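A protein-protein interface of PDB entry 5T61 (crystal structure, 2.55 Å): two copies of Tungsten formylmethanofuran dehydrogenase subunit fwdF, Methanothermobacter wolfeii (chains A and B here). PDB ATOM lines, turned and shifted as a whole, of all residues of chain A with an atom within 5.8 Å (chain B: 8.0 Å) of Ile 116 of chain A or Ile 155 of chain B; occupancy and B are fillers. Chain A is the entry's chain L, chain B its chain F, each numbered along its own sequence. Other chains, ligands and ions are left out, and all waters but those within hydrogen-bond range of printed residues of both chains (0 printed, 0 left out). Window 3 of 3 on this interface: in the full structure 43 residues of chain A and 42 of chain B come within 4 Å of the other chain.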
ATOM      1  N   ASP A 112       7.602   5.895 -22.614  1.00  0.00           N
ATOM      2  CA  ASP A 112       9.020   5.566 -22.663  1.00  0.00           C
ATOM      3  C   ASP A 112       9.517   5.343 -24.085  1.00  0.00           C
ATOM      4  O   ASP A 112      10.720   5.471 -24.334  1.00  0.00           O
ATOM      5  CB  ASP A 112       9.300   4.331 -21.806  1.00  0.00           C
ATOM      6  CG  ASP A 112       9.018   4.568 -20.336  1.00  0.00           C
ATOM      7  OD1 ASP A 112       9.622   5.494 -19.751  1.00  0.00           O
ATOM      8  OD2 ASP A 112       8.203   3.816 -19.762  1.00  0.00           O
ATOM      9  N   THR A 114       8.539   7.256 -26.624  1.00  0.00           N
ATOM     10  CA  THR A 114       8.738   8.610 -27.123  1.00  0.00           C
ATOM     11  C   THR A 114       9.933   9.269 -26.447  1.00  0.00           C
ATOM     12  O   THR A 114      10.686  10.013 -27.086  1.00  0.00           O
ATOM     13  CB  THR A 114       7.475   9.437 -26.878  1.00  0.00           C
ATOM     14  OG1 THR A 114       6.323   8.689 -27.292  1.00  0.00           O
ATOM     15  CG2 THR A 114       7.525  10.742 -27.656  1.00  0.00           C
ATOM     16  N   CYS A 115      10.102   8.998 -25.154  1.00  0.00           N
ATOM     17  CA  CYS A 115      11.185   9.545 -24.350  1.00  0.00           C
ATOM     18  C   CYS A 115      12.556   9.286 -24.971  1.00  0.00           C
ATOM     19  O   CYS A 115      12.856   8.169 -25.405  1.00  0.00           O
ATOM     20  CB  CYS A 115      11.093   8.927 -22.952  1.00  0.00           C
ATOM     21  SG  CYS A 115      12.583   8.969 -21.962  1.00  0.00           S
ATOM     22  N   ILE A 116      13.385  10.331 -25.010  1.00  0.00           N
ATOM     23  CA  ILE A 116      14.744  10.258 -25.539  1.00  0.00           C
ATOM     24  C   ILE A 116      15.787  10.464 -24.449  1.00  0.00           C
ATOM     25  O   ILE A 116      16.969  10.664 -24.758  1.00  0.00           O
ATOM     26  CB  ILE A 116      14.962  11.265 -26.681  1.00  0.00           C
ATOM     27  CG1 ILE A 116      14.812  12.698 -26.164  1.00  0.00           C
ATOM     28  CG2 ILE A 116      14.004  10.989 -27.828  1.00  0.00           C
ATOM     29  CD1 ILE A 116      15.221  13.750 -27.160  1.00  0.00           C
ATOM     30  N   GLN A 117      15.373  10.455 -23.178  1.00  0.00           N
ATOM     31  CA  GLN A 117      16.290  10.459 -22.039  1.00  0.00           C
ATOM     32  C   GLN A 117      17.098  11.753 -21.938  1.00  0.00           C
ATOM     33  O   GLN A 117      18.273  11.725 -21.569  1.00  0.00           O
ATOM     34  CB  GLN A 117      17.228   9.251 -22.092  1.00  0.00           C
ATOM     35  CG  GLN A 117      16.747   8.037 -21.334  1.00  0.00           C
ATOM     36  CD  GLN A 117      15.569   7.350 -21.965  1.00  0.00           C
ATOM     37  OE1 GLN A 117      14.637   6.943 -21.271  1.00  0.00           O
ATOM     38  NE2 GLN A 117      15.588   7.226 -23.285  1.00  0.00           N
ATOM     39  N   CYS A 118      16.475  12.895 -22.248  1.00  0.00           N
ATOM     40  CA  CYS A 118      17.205  14.155 -22.149  1.00  0.00           C
ATOM     41  C   CYS A 118      17.346  14.624 -20.705  1.00  0.00           C
ATOM     42  O   CYS A 118      18.231  15.441 -20.426  1.00  0.00           O
ATOM     43  CB  CYS A 118      16.549  15.250 -22.996  1.00  0.00           C
ATOM     44  SG  CYS A 118      15.349  16.309 -22.165  1.00  0.00           S
ATOM     45  N   ALA A 120      15.452  16.544 -18.793  1.00  0.00           N
ATOM     46  CA  ALA A 120      14.964  17.860 -18.379  1.00  0.00           C
ATOM     47  C   ALA A 120      13.921  17.741 -17.273  1.00  0.00           C
ATOM     48  O   ALA A 120      13.906  18.547 -16.332  1.00  0.00           O
ATOM     49  CB  ALA A 120      14.392  18.614 -19.579  1.00  0.00           C
ATOM     50  N   VAL A 228      20.923   5.555 -27.799  1.00  0.00           N
ATOM     51  CA  VAL A 228      21.004   5.829 -26.373  1.00  0.00           C
ATOM     52  C   VAL A 228      19.762   5.258 -25.702  1.00  0.00           C
ATOM     53  O   VAL A 228      18.636   5.655 -26.025  1.00  0.00           O
ATOM     54  CB  VAL A 228      21.132   7.340 -26.126  1.00  0.00           C
ATOM     55  CG1 VAL A 228      20.927   7.673 -24.654  1.00  0.00           C
ATOM     56  CG2 VAL A 228      22.488   7.832 -26.609  1.00  0.00           C
ATOM     57  N   PRO A 250      10.767  18.173 -24.295  1.00  0.00           N
ATOM     58  CA  PRO A 250      10.899  18.624 -25.689  1.00  0.00           C
ATOM     59  C   PRO A 250      10.194  17.729 -26.696  1.00  0.00           C
ATOM     60  O   PRO A 250       9.991  18.163 -27.836  1.00  0.00           O
ATOM     61  CB  PRO A 250      12.416  18.628 -25.913  1.00  0.00           C
ATOM     62  CG  PRO A 250      12.913  17.553 -25.008  1.00  0.00           C
ATOM     63  CD  PRO A 250      12.019  17.584 -23.789  1.00  0.00           C
ATOM     64  N   VAL A 251       9.814  16.504 -26.331  1.00  0.00           N
ATOM     65  CA  VAL A 251       9.150  15.620 -27.282  1.00  0.00           C
ATOM     66  C   VAL A 251       7.755  15.216 -26.801  1.00  0.00           C
ATOM     67  O   VAL A 251       7.193  14.241 -27.298  1.00  0.00           O
ATOM     68  CB  VAL A 251      10.009  14.379 -27.602  1.00  0.00           C
ATOM     69  CG1 VAL A 251      11.379  14.786 -28.156  1.00  0.00           C
ATOM     70  CG2 VAL A 251      10.129  13.453 -26.388  1.00  0.00           C
ATOM     71  N   ILE B 149      27.326  25.620 -32.131  1.00  0.00           N
ATOM     72  CA  ILE B 149      26.160  24.991 -31.531  1.00  0.00           C
ATOM     73  C   ILE B 149      24.968  25.912 -31.736  1.00  0.00           C
ATOM     74  O   ILE B 149      24.990  27.078 -31.321  1.00  0.00           O
ATOM     75  CB  ILE B 149      26.378  24.685 -30.041  1.00  0.00           C
ATOM     76  CG1 ILE B 149      27.671  23.894 -29.828  1.00  0.00           C
ATOM     77  CG2 ILE B 149      25.200  23.908 -29.489  1.00  0.00           C
ATOM     78  CD1 ILE B 149      27.761  23.285 -28.451  1.00  0.00           C
ATOM     79  N   ASP B 150      23.927  25.388 -32.374  1.00  0.00           N
ATOM     80  CA  ASP B 150      22.679  26.116 -32.542  1.00  0.00           C
ATOM     81  C   ASP B 150      21.869  25.992 -31.257  1.00  0.00           C
ATOM     82  O   ASP B 150      21.303  24.931 -30.972  1.00  0.00           O
ATOM     83  CB  ASP B 150      21.910  25.576 -33.741  1.00  0.00           C
ATOM     84  CG  ASP B 150      20.634  26.344 -34.008  1.00  0.00           C
ATOM     85  OD1 ASP B 150      20.413  27.395 -33.363  1.00  0.00           O
ATOM     86  OD2 ASP B 150      19.848  25.895 -34.866  1.00  0.00           O
ATOM     87  N   LYS B 151      21.822  27.071 -30.476  1.00  0.00           N
ATOM     88  CA  LYS B 151      21.193  27.017 -29.162  1.00  0.00           C
ATOM     89  C   LYS B 151      19.668  26.964 -29.237  1.00  0.00           C
ATOM     90  O   LYS B 151      19.033  26.541 -28.266  1.00  0.00           O
ATOM     91  CB  LYS B 151      21.673  28.197 -28.317  1.00  0.00           C
ATOM     92  CG  LYS B 151      23.176  28.413 -28.455  1.00  0.00           C
ATOM     93  CD  LYS B 151      23.679  29.632 -27.701  1.00  0.00           C
ATOM     94  CE  LYS B 151      25.194  29.760 -27.860  1.00  0.00           C
ATOM     95  NZ  LYS B 151      25.784  30.855 -27.036  1.00  0.00           N
ATOM     96  N   ASP B 152      19.066  27.370 -30.359  1.00  0.00           N
ATOM     97  CA  ASP B 152      17.617  27.231 -30.510  1.00  0.00           C
ATOM     98  C   ASP B 152      17.218  25.773 -30.715  1.00  0.00           C
ATOM     99  O   ASP B 152      16.213  25.316 -30.156  1.00  0.00           O
ATOM    100  CB  ASP B 152      17.123  28.075 -31.688  1.00  0.00           C
ATOM    101  CG  ASP B 152      17.451  29.548 -31.543  1.00  0.00           C
ATOM    102  OD1 ASP B 152      17.214  30.104 -30.450  1.00  0.00           O
ATOM    103  OD2 ASP B 152      17.989  30.137 -32.506  1.00  0.00           O
ATOM    104  N   THR B 153      18.002  25.024 -31.494  1.00  0.00           N
ATOM    105  CA  THR B 153      17.748  23.595 -31.657  1.00  0.00           C
ATOM    106  C   THR B 153      18.063  22.830 -30.377  1.00  0.00           C
ATOM    107  O   THR B 153      17.365  21.870 -30.027  1.00  0.00           O
ATOM    108  CB  THR B 153      18.577  23.046 -32.819  1.00  0.00           C
ATOM    109  OG1 THR B 153      18.305  23.803 -34.004  1.00  0.00           O
ATOM    110  CG2 THR B 153      18.257  21.584 -33.070  1.00  0.00           C
ATOM    111  N   CYS B 154      19.088  23.272 -29.659  1.00  0.00           N
ATOM    112  CA  CYS B 154      19.552  22.606 -28.453  1.00  0.00           C
ATOM    113  C   CYS B 154      18.433  22.455 -27.429  1.00  0.00           C
ATOM    114  O   CYS B 154      17.703  23.409 -27.139  1.00  0.00           O
ATOM    115  CB  CYS B 154      20.714  23.418 -27.876  1.00  0.00           C
ATOM    116  SG  CYS B 154      21.066  23.203 -26.134  1.00  0.00           S
ATOM    117  N   ILE B 155      18.297  21.243 -26.885  1.00  0.00           N
ATOM    118  CA  ILE B 155      17.312  20.953 -25.848  1.00  0.00           C
ATOM    119  C   ILE B 155      17.953  20.752 -24.488  1.00  0.00           C
ATOM    120  O   ILE B 155      17.245  20.410 -23.528  1.00  0.00           O
ATOM    121  CB  ILE B 155      16.455  19.726 -26.205  1.00  0.00           C
ATOM    122  CG1 ILE B 155      17.340  18.499 -26.429  1.00  0.00           C
ATOM    123  CG2 ILE B 155      15.631  20.005 -27.447  1.00  0.00           C
ATOM    124  CD1 ILE B 155      16.580  17.193 -26.424  1.00  0.00           C
ATOM    125  N   TYR B 156      19.271  20.949 -24.375  1.00  0.00           N
ATOM    126  CA  TYR B 156      19.977  20.939 -23.094  1.00  0.00           C
ATOM    127  C   TYR B 156      19.887  19.590 -22.385  1.00  0.00           C
ATOM    128  O   TYR B 156      19.635  19.509 -21.180  1.00  0.00           O
ATOM    129  CB  TYR B 156      19.481  22.075 -22.197  1.00  0.00           C
ATOM    130  CG  TYR B 156      19.874  23.435 -22.718  1.00  0.00           C
ATOM    131  CD1 TYR B 156      21.198  23.849 -22.667  1.00  0.00           C
ATOM    132  CD2 TYR B 156      18.944  24.279 -23.310  1.00  0.00           C
ATOM    133  CE1 TYR B 156      21.580  25.085 -23.146  1.00  0.00           C
ATOM    134  CE2 TYR B 156      19.319  25.519 -23.802  1.00  0.00           C
ATOM    135  CZ  TYR B 156      20.640  25.915 -23.717  1.00  0.00           C
ATOM    136  OH  TYR B 156      21.031  27.142 -24.200  1.00  0.00           O
ATOM    137  N   CYS B 157      20.103  18.519 -23.141  1.00  0.00           N
ATOM    138  CA  CYS B 157      20.125  17.192 -22.543  1.00  0.00           C
ATOM    139  C   CYS B 157      21.436  16.896 -21.824  1.00  0.00           C
ATOM    140  O   CYS B 157      21.509  15.907 -21.088  1.00  0.00           O
ATOM    141  CB  CYS B 157      19.865  16.130 -23.608  1.00  0.00           C
ATOM    142  SG  CYS B 157      21.308  15.628 -24.539  1.00  0.00           S
ATOM    143  N   GLY B 158      22.473  17.707 -22.036  1.00  0.00           N
ATOM    144  CA  GLY B 158      23.733  17.547 -21.340  1.00  0.00           C
ATOM    145  C   GLY B 158      24.652  16.472 -21.879  1.00  0.00           C
ATOM    146  O   GLY B 158      25.779  16.347 -21.386  1.00  0.00           O
ATOM    147  N   MET B 159      24.220  15.693 -22.876  1.00  0.00           N
ATOM    148  CA  MET B 159      25.005  14.535 -23.300  1.00  0.00           C
ATOM    149  C   MET B 159      26.333  14.944 -23.931  1.00  0.00           C
ATOM    150  O   MET B 159      27.342  14.249 -23.759  1.00  0.00           O
ATOM    151  CB  MET B 159      24.195  13.656 -24.256  1.00  0.00           C
ATOM    152  CG  MET B 159      23.072  12.849 -23.589  1.00  0.00           C
ATOM    153  SD  MET B 159      22.304  11.612 -24.674  1.00  0.00           S
ATOM    154  CE  MET B 159      20.821  12.404 -25.281  1.00  0.00           C
ATOM    155  N   ILE B 171      27.557  24.221 -19.958  1.00  0.00           N
ATOM    156  CA  ILE B 171      26.130  24.520 -19.961  1.00  0.00           C
ATOM    157  C   ILE B 171      25.788  25.238 -18.663  1.00  0.00           C
ATOM    158  O   ILE B 171      26.197  24.800 -17.582  1.00  0.00           O
ATOM    159  CB  ILE B 171      25.277  23.248 -20.125  1.00  0.00           C
ATOM    160  CG1 ILE B 171      25.493  22.629 -21.505  1.00  0.00           C
ATOM    161  CG2 ILE B 171      23.806  23.567 -19.939  1.00  0.00           C
ATOM    162  CD1 ILE B 171      24.914  21.240 -21.633  1.00  0.00           C
ATOM    163  N   VAL B 183      15.674  24.515 -18.129  1.00  0.00           N
ATOM    164  CA  VAL B 183      16.661  23.829 -17.298  1.00  0.00           C
ATOM    165  C   VAL B 183      18.068  24.343 -17.534  1.00  0.00           C
ATOM    166  O   VAL B 183      19.006  23.882 -16.869  1.00  0.00           O
ATOM    167  CB  VAL B 183      16.680  22.306 -17.546  1.00  0.00           C
ATOM    168  CG1 VAL B 183      15.305  21.697 -17.303  1.00  0.00           C
ATOM    169  CG2 VAL B 183      17.202  22.002 -18.947  1.00  0.00           C
ATOM    170  N   ALA B 184      18.246  25.272 -18.467  1.00  0.00           N
ATOM    171  CA  ALA B 184      19.538  25.879 -18.739  1.00  0.00           C
ATOM    172  C   ALA B 184      19.307  27.127 -19.573  1.00  0.00           C
ATOM    173  O   ALA B 184      18.325  27.216 -20.316  1.00  0.00           O
ATOM    174  CB  ALA B 184      20.477  24.911 -19.467  1.00  0.00           C
ATOM    175  N   ILE B 187      24.696  27.546 -23.628  1.00  0.00           N
ATOM    176  CA  ILE B 187      25.671  26.484 -23.857  1.00  0.00           C
ATOM    177  C   ILE B 187      26.817  27.057 -24.685  1.00  0.00           C
ATOM    178  O   ILE B 187      26.595  27.871 -25.588  1.00  0.00           O
ATOM    179  CB  ILE B 187      25.025  25.269 -24.559  1.00  0.00           C
ATOM    180  CG1 ILE B 187      26.052  24.161 -24.803  1.00  0.00           C
ATOM    181  CG2 ILE B 187      24.354  25.684 -25.862  1.00  0.00           C
ATOM    182  CD1 ILE B 187      25.437  22.860 -25.267  1.00  0.00           C
ATOM    183  N   CYS B 204      24.774  14.094 -30.062  1.00  0.00           N
ATOM    184  CA  CYS B 204      23.652  15.025 -30.006  1.00  0.00           C
ATOM    185  C   CYS B 204      22.376  14.427 -30.596  1.00  0.00           C
ATOM    186  O   CYS B 204      22.351  14.099 -31.793  1.00  0.00           O
ATOM    187  CB  CYS B 204      24.004  16.304 -30.755  1.00  0.00           C
ATOM    188  SG  CYS B 204      22.560  17.295 -31.188  1.00  0.00           S
ATOM    189  N   PRO B 205      21.299  14.289 -29.814  1.00  0.00           N
ATOM    190  CA  PRO B 205      20.069  13.674 -30.345  1.00  0.00           C
ATOM    191  C   PRO B 205      19.303  14.567 -31.313  1.00  0.00           C
ATOM    192  O   PRO B 205      18.410  14.066 -32.014  1.00  0.00           O
ATOM    193  CB  PRO B 205      19.245  13.391 -29.082  1.00  0.00           C
ATOM    194  CG  PRO B 205      19.697  14.438 -28.110  1.00  0.00           C
ATOM    195  CD  PRO B 205      21.157  14.692 -28.402  1.00  0.00           C
ATOM    196  N   VAL B 206      19.622  15.861 -31.381  1.00  0.00           N
ATOM    197  CA  VAL B 206      18.883  16.813 -32.196  1.00  0.00           C
ATOM    198  C   VAL B 206      19.754  17.460 -33.267  1.00  0.00           C
ATOM    199  O   VAL B 206      19.332  18.436 -33.889  1.00  0.00           O
ATOM    200  CB  VAL B 206      18.228  17.901 -31.319  1.00  0.00           C
ATOM    201  CG1 VAL B 206      17.204  17.286 -30.378  1.00  0.00           C
ATOM    202  CG2 VAL B 206      19.296  18.634 -30.508  1.00  0.00           C
ATOM    203  N   ALA B 208      22.209  19.445 -33.260  1.00  0.00           N
ATOM    204  CA  ALA B 208      22.329  20.878 -33.047  1.00  0.00           C
ATOM    205  C   ALA B 208      23.764  21.365 -33.135  1.00  0.00           C
ATOM    206  O   ALA B 208      23.996  22.578 -33.089  1.00  0.00           O
ATOM    207  CB  ALA B 208      21.740  21.266 -31.686  1.00  0.00           C
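The backbone carbonyl oxygen (O) of Cys 157 of chain B sits close to the backbone carbonyl oxygen (O) of Cys 118 of chain A.
The backbone NH (N) of Met 159 of chain B sits close to the side-chain sulfur (SG) of Cys 157 of chain B, at 3.4 Å. N of Ala 120 of chain A sits close to SG of Cys 118 of chain A.
CD1 of Ile 116 of chain A touches CD1 of Ile 155 of chain B, 3.8 Å away. CB of Cys 118 of chain A touches CD1 of Ile 155 of chain B, 3.9 Å away. Ala 120 of chain A touches Val 183 of chain B (O to CG1, 3.6 Å). CB of Pro 250 of chain A touches CG2 of Ile 155 of chain B, 3.8 Å away.
Asp 112 of chain A touches none of the printed residues of chain B. Of chain B, only Ile 155 (3.8 Å) comes within 4 Å of Ile 116 of chain A. Printed residues of chain A within 4 Å of Cys 157 of chain B: Cys 118. Of the printed residues of chain A, Val 183 of chain B touches Ala 120 (3.6 Å). The nearest residue of chain B that does not touch Ile 116 of chain A is Met 159 of chain B (4.3 Å). The nearest residue of chain A that does not touch Ile 155 of chain B is Ala 120 of chain A (5.2 Å).
Of the 10 printed residues of chain A, 4 touch a printed residue of chain B. Among the printed residues, 5 pairs touch across the chains. Among the printed residues, no Asp or Glu carboxylate lies within 4 Å of a Lys or Arg side-chain nitrogen of the other chain.
No position is printed for both chains.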
